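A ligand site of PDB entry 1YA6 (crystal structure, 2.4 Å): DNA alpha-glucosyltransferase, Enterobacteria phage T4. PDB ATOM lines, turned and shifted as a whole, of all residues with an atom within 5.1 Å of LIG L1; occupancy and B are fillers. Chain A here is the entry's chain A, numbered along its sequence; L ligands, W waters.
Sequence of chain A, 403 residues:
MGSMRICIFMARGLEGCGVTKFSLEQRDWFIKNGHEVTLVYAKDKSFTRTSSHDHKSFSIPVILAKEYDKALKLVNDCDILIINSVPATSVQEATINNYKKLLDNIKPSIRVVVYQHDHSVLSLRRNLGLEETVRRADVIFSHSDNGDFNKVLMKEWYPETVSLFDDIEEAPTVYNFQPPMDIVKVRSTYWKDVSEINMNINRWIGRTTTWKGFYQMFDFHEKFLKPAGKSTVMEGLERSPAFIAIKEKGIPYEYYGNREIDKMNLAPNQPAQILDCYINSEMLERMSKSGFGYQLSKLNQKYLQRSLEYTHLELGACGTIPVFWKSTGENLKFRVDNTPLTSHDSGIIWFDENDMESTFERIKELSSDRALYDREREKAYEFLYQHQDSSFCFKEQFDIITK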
ATOM      1  N   GLY A  16      21.360   8.064 -12.183  1.00  0.00           N
ATOM      2  CA  GLY A  16      22.341   8.105 -13.254  1.00  0.00           C
ATOM      3  C   GLY A  16      23.785   7.815 -12.888  1.00  0.00           C
ATOM      4  O   GLY A  16      24.704   8.168 -13.616  1.00  0.00           O
ATOM      5  N   CYS A  17      23.981   7.148 -11.768  1.00  0.00           N
ATOM      6  CA  CYS A  17      25.323   6.832 -11.347  1.00  0.00           C
ATOM      7  C   CYS A  17      25.492   5.331 -11.180  1.00  0.00           C
ATOM      8  O   CYS A  17      25.048   4.545 -12.034  1.00  0.00           O
ATOM      9  CB  CYS A  17      25.672   7.548 -10.058  1.00  0.00           C
ATOM     10  SG  CYS A  17      25.531   9.346 -10.164  1.00  0.00           S
ATOM     11  N   GLY A  18      26.137   4.945 -10.092  1.00  0.00           N
ATOM     12  CA  GLY A  18      26.406   3.549  -9.848  1.00  0.00           C
ATOM     13  C   GLY A  18      25.213   2.654  -9.612  1.00  0.00           C
ATOM     14  O   GLY A  18      25.253   1.488  -9.950  1.00  0.00           O
ATOM     15  N   VAL A  19      24.167   3.192  -8.994  1.00  0.00           N
ATOM     16  CA  VAL A  19      23.004   2.373  -8.726  1.00  0.00           C
ATOM     17  C   VAL A  19      22.236   2.168 -10.050  1.00  0.00           C
ATOM     18  O   VAL A  19      21.734   1.090 -10.323  1.00  0.00           O
ATOM     19  CB  VAL A  19      22.105   3.023  -7.625  1.00  0.00           C
ATOM     20  CG1 VAL A  19      20.993   2.092  -7.220  1.00  0.00           C
ATOM     21  CG2 VAL A  19      22.971   3.348  -6.401  1.00  0.00           C
ATOM     22  N   LYS A  21      23.656   2.353 -12.988  1.00  0.00           N
ATOM     23  CA  LYS A  21      24.568   1.525 -13.765  1.00  0.00           C
ATOM     24  C   LYS A  21      24.379   0.088 -13.318  1.00  0.00           C
ATOM     25  O   LYS A  21      24.023  -0.766 -14.118  1.00  0.00           O
ATOM     26  CB  LYS A  21      26.012   1.951 -13.537  1.00  0.00           C
ATOM     27  CG  LYS A  21      27.056   1.097 -14.260  1.00  0.00           C
ATOM     28  CD  LYS A  21      27.014   1.272 -15.762  1.00  0.00           C
ATOM     29  CE  LYS A  21      28.236   0.634 -16.404  1.00  0.00           C
ATOM     30  NZ  LYS A  21      28.114   0.516 -17.878  1.00  0.00           N
ATOM     31  N   ARG A  49      21.776  13.457 -13.963  1.00  0.00           N
ATOM     32  CA  ARG A  49      22.397  12.527 -14.884  1.00  0.00           C
ATOM     33  C   ARG A  49      21.422  11.508 -15.485  1.00  0.00           C
ATOM     34  O   ARG A  49      21.811  10.405 -15.882  1.00  0.00           O
ATOM     35  CB  ARG A  49      23.559  11.841 -14.185  1.00  0.00           C
ATOM     36  CG  ARG A  49      24.583  12.856 -13.711  1.00  0.00           C
ATOM     37  CD  ARG A  49      25.706  12.235 -12.926  1.00  0.00           C
ATOM     38  NE  ARG A  49      25.984  13.078 -11.774  1.00  0.00           N
ATOM     39  CZ  ARG A  49      27.086  13.805 -11.619  1.00  0.00           C
ATOM     40  NH1 ARG A  49      28.029  13.807 -12.557  1.00  0.00           N
ATOM     41  NH2 ARG A  49      27.221  14.555 -10.537  1.00  0.00           N
ATOM     42  N   SER A  52      22.699  10.013 -18.619  1.00  0.00           N
ATOM     43  CA  SER A  52      24.067   9.508 -18.665  1.00  0.00           C
ATOM     44  C   SER A  52      24.201   8.078 -19.149  1.00  0.00           C
ATOM     45  O   SER A  52      25.227   7.690 -19.704  1.00  0.00           O
ATOM     46  CB  SER A  52      24.735   9.657 -17.284  1.00  0.00           C
ATOM     47  OG  SER A  52      24.991  11.023 -17.016  1.00  0.00           O
ATOM     48  N   HIS A  53      23.160   7.283 -18.926  1.00  0.00           N
ATOM     49  CA  HIS A  53      23.157   5.894 -19.372  1.00  0.00           C
ATOM     50  C   HIS A  53      21.952   5.735 -20.278  1.00  0.00           C
ATOM     51  O   HIS A  53      20.976   6.485 -20.178  1.00  0.00           O
ATOM     52  CB  HIS A  53      23.064   4.938 -18.190  1.00  0.00           C
ATOM     53  CG  HIS A  53      24.224   5.013 -17.241  1.00  0.00           C
ATOM     54  ND1 HIS A  53      24.283   5.905 -16.204  1.00  0.00           N
ATOM     55  CD2 HIS A  53      25.405   4.333 -17.227  1.00  0.00           C
ATOM     56  CE1 HIS A  53      25.450   5.781 -15.580  1.00  0.00           C
ATOM     57  NE2 HIS A  53      26.145   4.837 -16.191  1.00  0.00           N
ATOM     58  N   GLY A 206      34.673  11.135 -12.523  1.00  0.00           N
ATOM     59  CA  GLY A 206      34.038  10.959 -11.235  1.00  0.00           C
ATOM     60  C   GLY A 206      32.995  12.051 -11.069  1.00  0.00           C
ATOM     61  O   GLY A 206      32.300  12.409 -12.028  1.00  0.00           O
ATOM     62  N   ARG A 207      32.854  12.570  -9.853  1.00  0.00           N
ATOM     63  CA  ARG A 207      31.894  13.647  -9.635  1.00  0.00           C
ATOM     64  C   ARG A 207      32.328  14.536  -8.493  1.00  0.00           C
ATOM     65  O   ARG A 207      33.317  14.245  -7.817  1.00  0.00           O
ATOM     66  CB  ARG A 207      30.482  13.107  -9.407  1.00  0.00           C
ATOM     67  CG  ARG A 207      30.339  11.925  -8.504  1.00  0.00           C
ATOM     68  CD  ARG A 207      28.872  11.519  -8.451  1.00  0.00           C
ATOM     69  NE  ARG A 207      28.652  10.442  -7.500  1.00  0.00           N
ATOM     70  CZ  ARG A 207      28.722  10.572  -6.177  1.00  0.00           C
ATOM     71  NH1 ARG A 207      28.507   9.521  -5.397  1.00  0.00           N
ATOM     72  NH2 ARG A 207      28.979  11.759  -5.638  1.00  0.00           N
ATOM     73  N   TRP A 211      35.858  12.694  -1.739  1.00  0.00           N
ATOM     74  CA  TRP A 211      36.534  11.395  -1.767  1.00  0.00           C
ATOM     75  C   TRP A 211      36.749  10.812  -3.185  1.00  0.00           C
ATOM     76  O   TRP A 211      37.323   9.730  -3.321  1.00  0.00           O
ATOM     77  CB  TRP A 211      35.831  10.381  -0.870  1.00  0.00           C
ATOM     78  CG  TRP A 211      34.375  10.229  -1.117  1.00  0.00           C
ATOM     79  CD1 TRP A 211      33.378  11.012  -0.612  1.00  0.00           C
ATOM     80  CD2 TRP A 211      33.741   9.233  -1.930  1.00  0.00           C
ATOM     81  NE1 TRP A 211      32.159  10.568  -1.061  1.00  0.00           N
ATOM     82  CE2 TRP A 211      32.347   9.481  -1.874  1.00  0.00           C
ATOM     83  CE3 TRP A 211      34.204   8.164  -2.716  1.00  0.00           C
ATOM     84  CZ2 TRP A 211      31.415   8.691  -2.570  1.00  0.00           C
ATOM     85  CZ3 TRP A 211      33.294   7.382  -3.404  1.00  0.00           C
ATOM     86  CH2 TRP A 211      31.913   7.645  -3.322  1.00  0.00           C
ATOM     87  N   LYS A 212      36.303  11.508  -4.218  1.00  0.00           N
ATOM     88  CA  LYS A 212      36.536  11.031  -5.585  1.00  0.00           C
ATOM     89  C   LYS A 212      37.947  11.496  -5.968  1.00  0.00           C
ATOM     90  O   LYS A 212      38.468  11.177  -7.029  1.00  0.00           O
ATOM     91  CB  LYS A 212      35.518  11.639  -6.563  1.00  0.00           C
ATOM     92  CG  LYS A 212      34.076  11.180  -6.371  1.00  0.00           C
ATOM     93  CD  LYS A 212      33.912   9.692  -6.583  1.00  0.00           C
ATOM     94  CE  LYS A 212      32.439   9.282  -6.625  1.00  0.00           C
ATOM     95  NZ  LYS A 212      32.297   7.826  -6.971  1.00  0.00           N
ATOM     96  N   GLY A 236      32.689  14.986 -15.502  1.00  0.00           N
ATOM     97  CA  GLY A 236      31.709  14.697 -14.481  1.00  0.00           C
ATOM     98  C   GLY A 236      31.525  15.673 -13.343  1.00  0.00           C
ATOM     99  O   GLY A 236      30.580  15.509 -12.565  1.00  0.00           O
ATOM    100  N   ASP A 276      31.220  18.731 -17.486  1.00  0.00           N
ATOM    101  CA  ASP A 276      30.266  18.369 -16.440  1.00  0.00           C
ATOM    102  C   ASP A 276      29.621  17.011 -16.689  1.00  0.00           C
ATOM    103  O   ASP A 276      30.172  16.190 -17.429  1.00  0.00           O
ATOM    104  CB  ASP A 276      29.187  19.441 -16.257  1.00  0.00           C
ATOM    105  CG  ASP A 276      28.223  19.530 -17.411  1.00  0.00           C
ATOM    106  OD1 ASP A 276      27.242  20.306 -17.297  1.00  0.00           O
ATOM    107  OD2 ASP A 276      28.445  18.816 -18.417  1.00  0.00           O
ATOM    108  N   CYS A 277      28.472  16.764 -16.074  1.00  0.00           N
ATOM    109  CA  CYS A 277      27.787  15.486 -16.263  1.00  0.00           C
ATOM    110  C   CYS A 277      27.890  15.058 -17.712  1.00  0.00           C
ATOM    111  O   CYS A 277      27.411  15.733 -18.616  1.00  0.00           O
ATOM    112  CB  CYS A 277      26.348  15.604 -15.831  1.00  0.00           C
ATOM    113  SG  CYS A 277      26.300  16.160 -14.146  1.00  0.00           S
ATOM    114  N   TYR A 278      28.530  13.923 -17.906  1.00  0.00           N
ATOM    115  CA  TYR A 278      28.787  13.377 -19.234  1.00  0.00           C
ATOM    116  C   TYR A 278      28.010  12.090 -19.566  1.00  0.00           C
ATOM    117  O   TYR A 278      27.523  11.389 -18.665  1.00  0.00           O
ATOM    118  CB  TYR A 278      30.278  13.108 -19.324  1.00  0.00           C
ATOM    119  CG  TYR A 278      30.720  12.001 -18.396  1.00  0.00           C
ATOM    120  CD1 TYR A 278      30.435  10.672 -18.671  1.00  0.00           C
ATOM    121  CD2 TYR A 278      31.444  12.288 -17.236  1.00  0.00           C
ATOM    122  CE1 TYR A 278      30.860   9.659 -17.841  1.00  0.00           C
ATOM    123  CE2 TYR A 278      31.875  11.276 -16.399  1.00  0.00           C
ATOM    124  CZ  TYR A 278      31.592   9.969 -16.702  1.00  0.00           C
ATOM    125  OH  TYR A 278      32.051   8.962 -15.900  1.00  0.00           O
ATOM    126  N   ILE A 279      27.921  11.803 -20.858  1.00  0.00           N
ATOM    127  CA  ILE A 279      27.241  10.606 -21.361  1.00  0.00           C
ATOM    128  C   ILE A 279      28.226   9.442 -21.185  1.00  0.00           C
ATOM    129  O   ILE A 279      29.368   9.541 -21.615  1.00  0.00           O
ATOM    130  CB  ILE A 279      26.923  10.761 -22.854  1.00  0.00           C
ATOM    131  CG1 ILE A 279      26.178  12.080 -23.078  1.00  0.00           C
ATOM    132  CG2 ILE A 279      26.139   9.571 -23.342  1.00  0.00           C
ATOM    133  CD1 ILE A 279      24.784  12.086 -22.555  1.00  0.00           C
ATOM    134  N   ASN A 280      27.795   8.346 -20.589  1.00  0.00           N
ATOM    135  CA  ASN A 280      28.692   7.227 -20.362  1.00  0.00           C
ATOM    136  C   ASN A 280      29.347   6.655 -21.612  1.00  0.00           C
ATOM    137  O   ASN A 280      30.545   6.382 -21.616  1.00  0.00           O
ATOM    138  CB  ASN A 280      27.998   6.089 -19.598  1.00  0.00           C
ATOM    139  CG  ASN A 280      28.963   4.965 -19.221  1.00  0.00           C
ATOM    140  OD1 ASN A 280      28.937   3.883 -19.808  1.00  0.00           O
ATOM    141  ND2 ASN A 280      29.849   5.234 -18.259  1.00  0.00           N
ATOM    142  N   MET A 283      31.938   8.993 -23.083  1.00  0.00           N
ATOM    143  CA  MET A 283      33.103   9.024 -22.209  1.00  0.00           C
ATOM    144  C   MET A 283      34.017   7.864 -22.497  1.00  0.00           C
ATOM    145  O   MET A 283      35.235   8.019 -22.548  1.00  0.00           O
ATOM    146  CB  MET A 283      32.660   8.992 -20.742  1.00  0.00           C
ATOM    147  CG  MET A 283      33.786   9.134 -19.698  1.00  0.00           C
ATOM    148  SD  MET A 283      34.802   7.685 -19.490  1.00  0.00           S
ATOM    149  CE  MET A 283      33.698   6.565 -18.654  1.00  0.00           C
ATOM    150  N   GLU A 309      34.513   0.552  -7.881  1.00  0.00           N
ATOM    151  CA  GLU A 309      33.435   1.367  -8.430  1.00  0.00           C
ATOM    152  C   GLU A 309      33.367   1.298  -9.950  1.00  0.00           C
ATOM    153  O   GLU A 309      34.380   1.095 -10.616  1.00  0.00           O
ATOM    154  CB  GLU A 309      33.618   2.806  -8.000  1.00  0.00           C
ATOM    155  CG  GLU A 309      33.633   2.966  -6.499  1.00  0.00           C
ATOM    156  CD  GLU A 309      33.724   4.413  -6.076  1.00  0.00           C
ATOM    157  OE1 GLU A 309      34.833   4.987  -6.163  1.00  0.00           O
ATOM    158  OE2 GLU A 309      32.680   4.982  -5.690  1.00  0.00           O
ATOM    159  N   TYR A 310      32.180   1.486 -10.514  1.00  0.00           N
ATOM    160  CA  TYR A 310      32.041   1.424 -11.956  1.00  0.00           C
ATOM    161  C   TYR A 310      33.125   2.160 -12.737  1.00  0.00           C
ATOM    162  O   TYR A 310      33.668   1.608 -13.701  1.00  0.00           O
ATOM    163  CB  TYR A 310      30.647   1.885 -12.390  1.00  0.00           C
ATOM    164  CG  TYR A 310      29.676   0.757 -12.161  1.00  0.00           C
ATOM    165  CD1 TYR A 310      28.658   0.838 -11.213  1.00  0.00           C
ATOM    166  CD2 TYR A 310      29.889  -0.456 -12.791  1.00  0.00           C
ATOM    167  CE1 TYR A 310      27.892  -0.278 -10.888  1.00  0.00           C
ATOM    168  CE2 TYR A 310      29.140  -1.570 -12.480  1.00  0.00           C
ATOM    169  CZ  TYR A 310      28.157  -1.496 -11.533  1.00  0.00           C
ATOM    170  OH  TYR A 310      27.498  -2.656 -11.197  1.00  0.00           O
ATOM    171  N   THR A 311      33.463   3.387 -12.328  1.00  0.00           N
ATOM    172  CA  THR A 311      34.496   4.156 -13.035  1.00  0.00           C
ATOM    173  C   THR A 311      35.852   3.484 -12.928  1.00  0.00           C
ATOM    174  O   THR A 311      36.746   3.762 -13.718  1.00  0.00           O
ATOM    175  CB  THR A 311      34.618   5.593 -12.508  1.00  0.00           C
ATOM    176  OG1 THR A 311      34.766   5.562 -11.089  1.00  0.00           O
ATOM    177  CG2 THR A 311      33.408   6.413 -12.918  1.00  0.00           C
ATOM    178  N   GLU A 314      35.603   0.765 -15.676  1.00  0.00           N
ATOM    179  CA  GLU A 314      35.448   1.333 -17.007  1.00  0.00           C
ATOM    180  C   GLU A 314      36.770   1.791 -17.600  1.00  0.00           C
ATOM    181  O   GLU A 314      36.871   2.038 -18.802  1.00  0.00           O
ATOM    182  CB  GLU A 314      34.479   2.510 -16.969  1.00  0.00           C
ATOM    183  CG  GLU A 314      33.019   2.087 -16.970  1.00  0.00           C
ATOM    184  CD  GLU A 314      32.066   3.223 -16.649  1.00  0.00           C
ATOM    185  OE1 GLU A 314      30.892   3.139 -17.069  1.00  0.00           O
ATOM    186  OE2 GLU A 314      32.485   4.188 -15.972  1.00  0.00           O
HETATM  187  N1  LIG L   1      28.799   8.403 -14.956  1.00  0.00           N
HETATM  188  C1  LIG L   1      28.248   8.917 -16.117  1.00  0.00           C
HETATM  189  N2  LIG L   1      28.180  10.278 -16.170  1.00  0.00           N
HETATM  190  C2  LIG L   1      28.626  11.176 -15.215  1.00  0.00           C
HETATM  191  C3  LIG L   1      29.212  10.568 -14.059  1.00  0.00           C
HETATM  192  C4  LIG L   1      29.281   9.234 -13.984  1.00  0.00           C
HETATM  193  O1  LIG L   1      27.854   8.203 -17.017  1.00  0.00           O
HETATM  194  O2  LIG L   1      28.476  12.391 -15.404  1.00  0.00           O
HETATM  195  C5  LIG L   1      28.828   6.945 -14.826  1.00  0.00           C
HETATM  196  C6  LIG L   1      30.204   6.377 -14.518  1.00  0.00           C
HETATM  197  O3  LIG L   1      30.882   6.098 -15.728  1.00  0.00           O
HETATM  198  C7  LIG L   1      29.841   5.118 -13.729  1.00  0.00           C
HETATM  199  C8  LIG L   1      28.594   5.542 -12.958  1.00  0.00           C
HETATM  200  O4  LIG L   1      28.001   6.610 -13.728  1.00  0.00           O
HETATM  201  O5  LIG L   1      29.539   4.065 -14.626  1.00  0.00           O
HETATM  202  C9  LIG L   1      28.835   6.018 -11.550  1.00  0.00           C
HETATM  203  O6  LIG L   1      29.102   4.922 -10.691  1.00  0.00           O
HETATM  204  P1  LIG L   1      30.421   4.846  -9.810  1.00  0.00           P
HETATM  205  O7  LIG L   1      30.364   3.579  -9.027  1.00  0.00           O
HETATM  206  O8  LIG L   1      31.586   5.107 -10.704  1.00  0.00           O
HETATM  207  O9  LIG L   1      30.343   6.110  -8.770  1.00  0.00           O
HETATM  208  P2  LIG L   1      29.064   6.838  -8.044  1.00  0.00           P
HETATM  209  O10 LIG L   1      29.474   7.114  -6.643  1.00  0.00           O
HETATM  210  O11 LIG L   1      28.637   7.969  -8.910  1.00  0.00           O
HETATM  211  O12 LIG L   1      27.919   5.740  -8.038  1.00  0.00           O
HETATM  212 CO1  LG2 L   2      28.865   3.804  -4.794  1.00  0.00          CO
HETATM  213  N1  LG2 L   2      29.592   4.286  -6.589  1.00  0.00           N
HETATM  214  N2  LG2 L   2      29.276   1.876  -5.160  1.00  0.00           N
HETATM  215  N3  LG2 L   2      30.689   4.069  -4.070  1.00  0.00           N
HETATM  216  N4  LG2 L   2      28.178   3.306  -2.990  1.00  0.00           N
HETATM  217  N5  LG2 L   2      28.427   5.737  -4.434  1.00  0.00           N
HETATM  218  N6  LG2 L   2      27.029   3.565  -5.588  1.00  0.00           N
HETATM  219  O   HOH W   1      30.844   8.599 -10.261  1.00  0.00           O
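O3 of LIG L1 is in hydrogen-bond range of OE2 of Glu 314 (2.5 Å).
The backbone NH (N) of Tyr 278 lies within hydrogen-bond range of an oxygen (O2) of LIG L1 (2.9 Å).
A nitrogen (N2) of LIG L1 sits at hydrogen-bond distance from the backbone carbonyl oxygen (O) of Tyr 278 (2.8 Å).
OH of Tyr 278 lies within hydrogen-bond range of O3 of LIG L1, 3.1 Å away.
The backbone NH (N) of Gly 18 sits at hydrogen-bond distance from an oxygen (O12) of LIG L1, at 2.8 Å.
The guanidinium group (NE) of Arg 207 is in salt-bridge range of an oxygen (O11) of LIG L1.
An oxygen (O3) of LIG L1 sits at hydrogen-bond distance from the side-chain amide nitrogen of Asn 280 (2.9 Å).
An oxygen (O10) of LIG L1 lies within salt-bridge range of the side-chain amino group of Lys 212.
The backbone NH of Thr 311 lies within hydrogen-bond range of an oxygen (O8) of LIG L1.
OG1 of Thr 311 lies close to O8 of LIG L1 (3.2 Å).
An oxygen (O7) of LIG L1 sits at hydrogen-bond distance from the backbone NH (N) of Tyr 310 (3.1 Å).
SG of Cys 17 sits close to O11 of LIG L1 (3.6 Å).
An oxygen (O2) of LIG L1 sits at hydrogen-bond distance from the guanidinium group (NH1) of Arg 49, at 3.2 Å.
The side-chain hydroxyl (OG) of Ser 52 lies within hydrogen-bond range of a nitrogen (N2) of LIG L1 (3.4 Å).
A nitrogen (N3) of LG2 L2 lies close to the side-chain carboxylate (OE2) of Glu 309, at 2.7 Å.
An oxygen (O12) of LIG L1 sits close to a nitrogen (N1) of LG2 L2 (2.6 Å).
The side-chain carboxylate of Glu 314 lies within hydrogen-bond range of the side-chain amide nitrogen of Asn 280, 2.6 Å away.
The side-chain carboxylate (OE1) of Glu 314 is in salt-bridge range of the side-chain amino group (NZ) of Lys 21, 3.9 Å away.
The backbone carbonyl oxygen (O) of Tyr 278 is in hydrogen-bond range of the side-chain hydroxyl (OG) of Ser 52 (3.0 Å).
N of Asn 280 sits at hydrogen-bond distance from O of Ser 52, 2.8 Å away.
The guanidinium group (NH1) of Arg 49 lies within hydrogen-bond range of the side-chain sulfur (SG) of Cys 277 (3.3 Å).
The side-chain hydroxyl of Ser 52 sits close to the backbone carbonyl oxygen of Arg 49.
NH1 of Arg 49 sits at hydrogen-bond distance from O of Gly 236.
A ring nitrogen (ND1) of His 53 lies close to the backbone carbonyl oxygen of Gly 16 (3.5 Å).
Gly 16 touches LIG L1.
CG of Lys 21 touches O5 of LIG L1, at 3.9 Å.
His 53 touches LIG L1.
Cys 277 touches LIG L1 (CA to O2, 3.3 Å).
CB of Glu 309 touches O7 of LIG L1, at 3.5 Å.
Hydrophobic or aromatic side chains that line LIG L1: His 53, Tyr 278 and Tyr 310.
16 residues have an atom within 4 Å of LIG L1: Gly 16, Cys 17, Gly 18, Lys 21, Arg 49, Ser 52, His 53, Arg 207, Lys 212, Cys 277, Tyr 278, Asn 280, Glu 309, Tyr 310, Thr 311 and Glu 314.
The nearest printed residue that does not touch LIG L1 is Gly 236 (4.1 Å).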
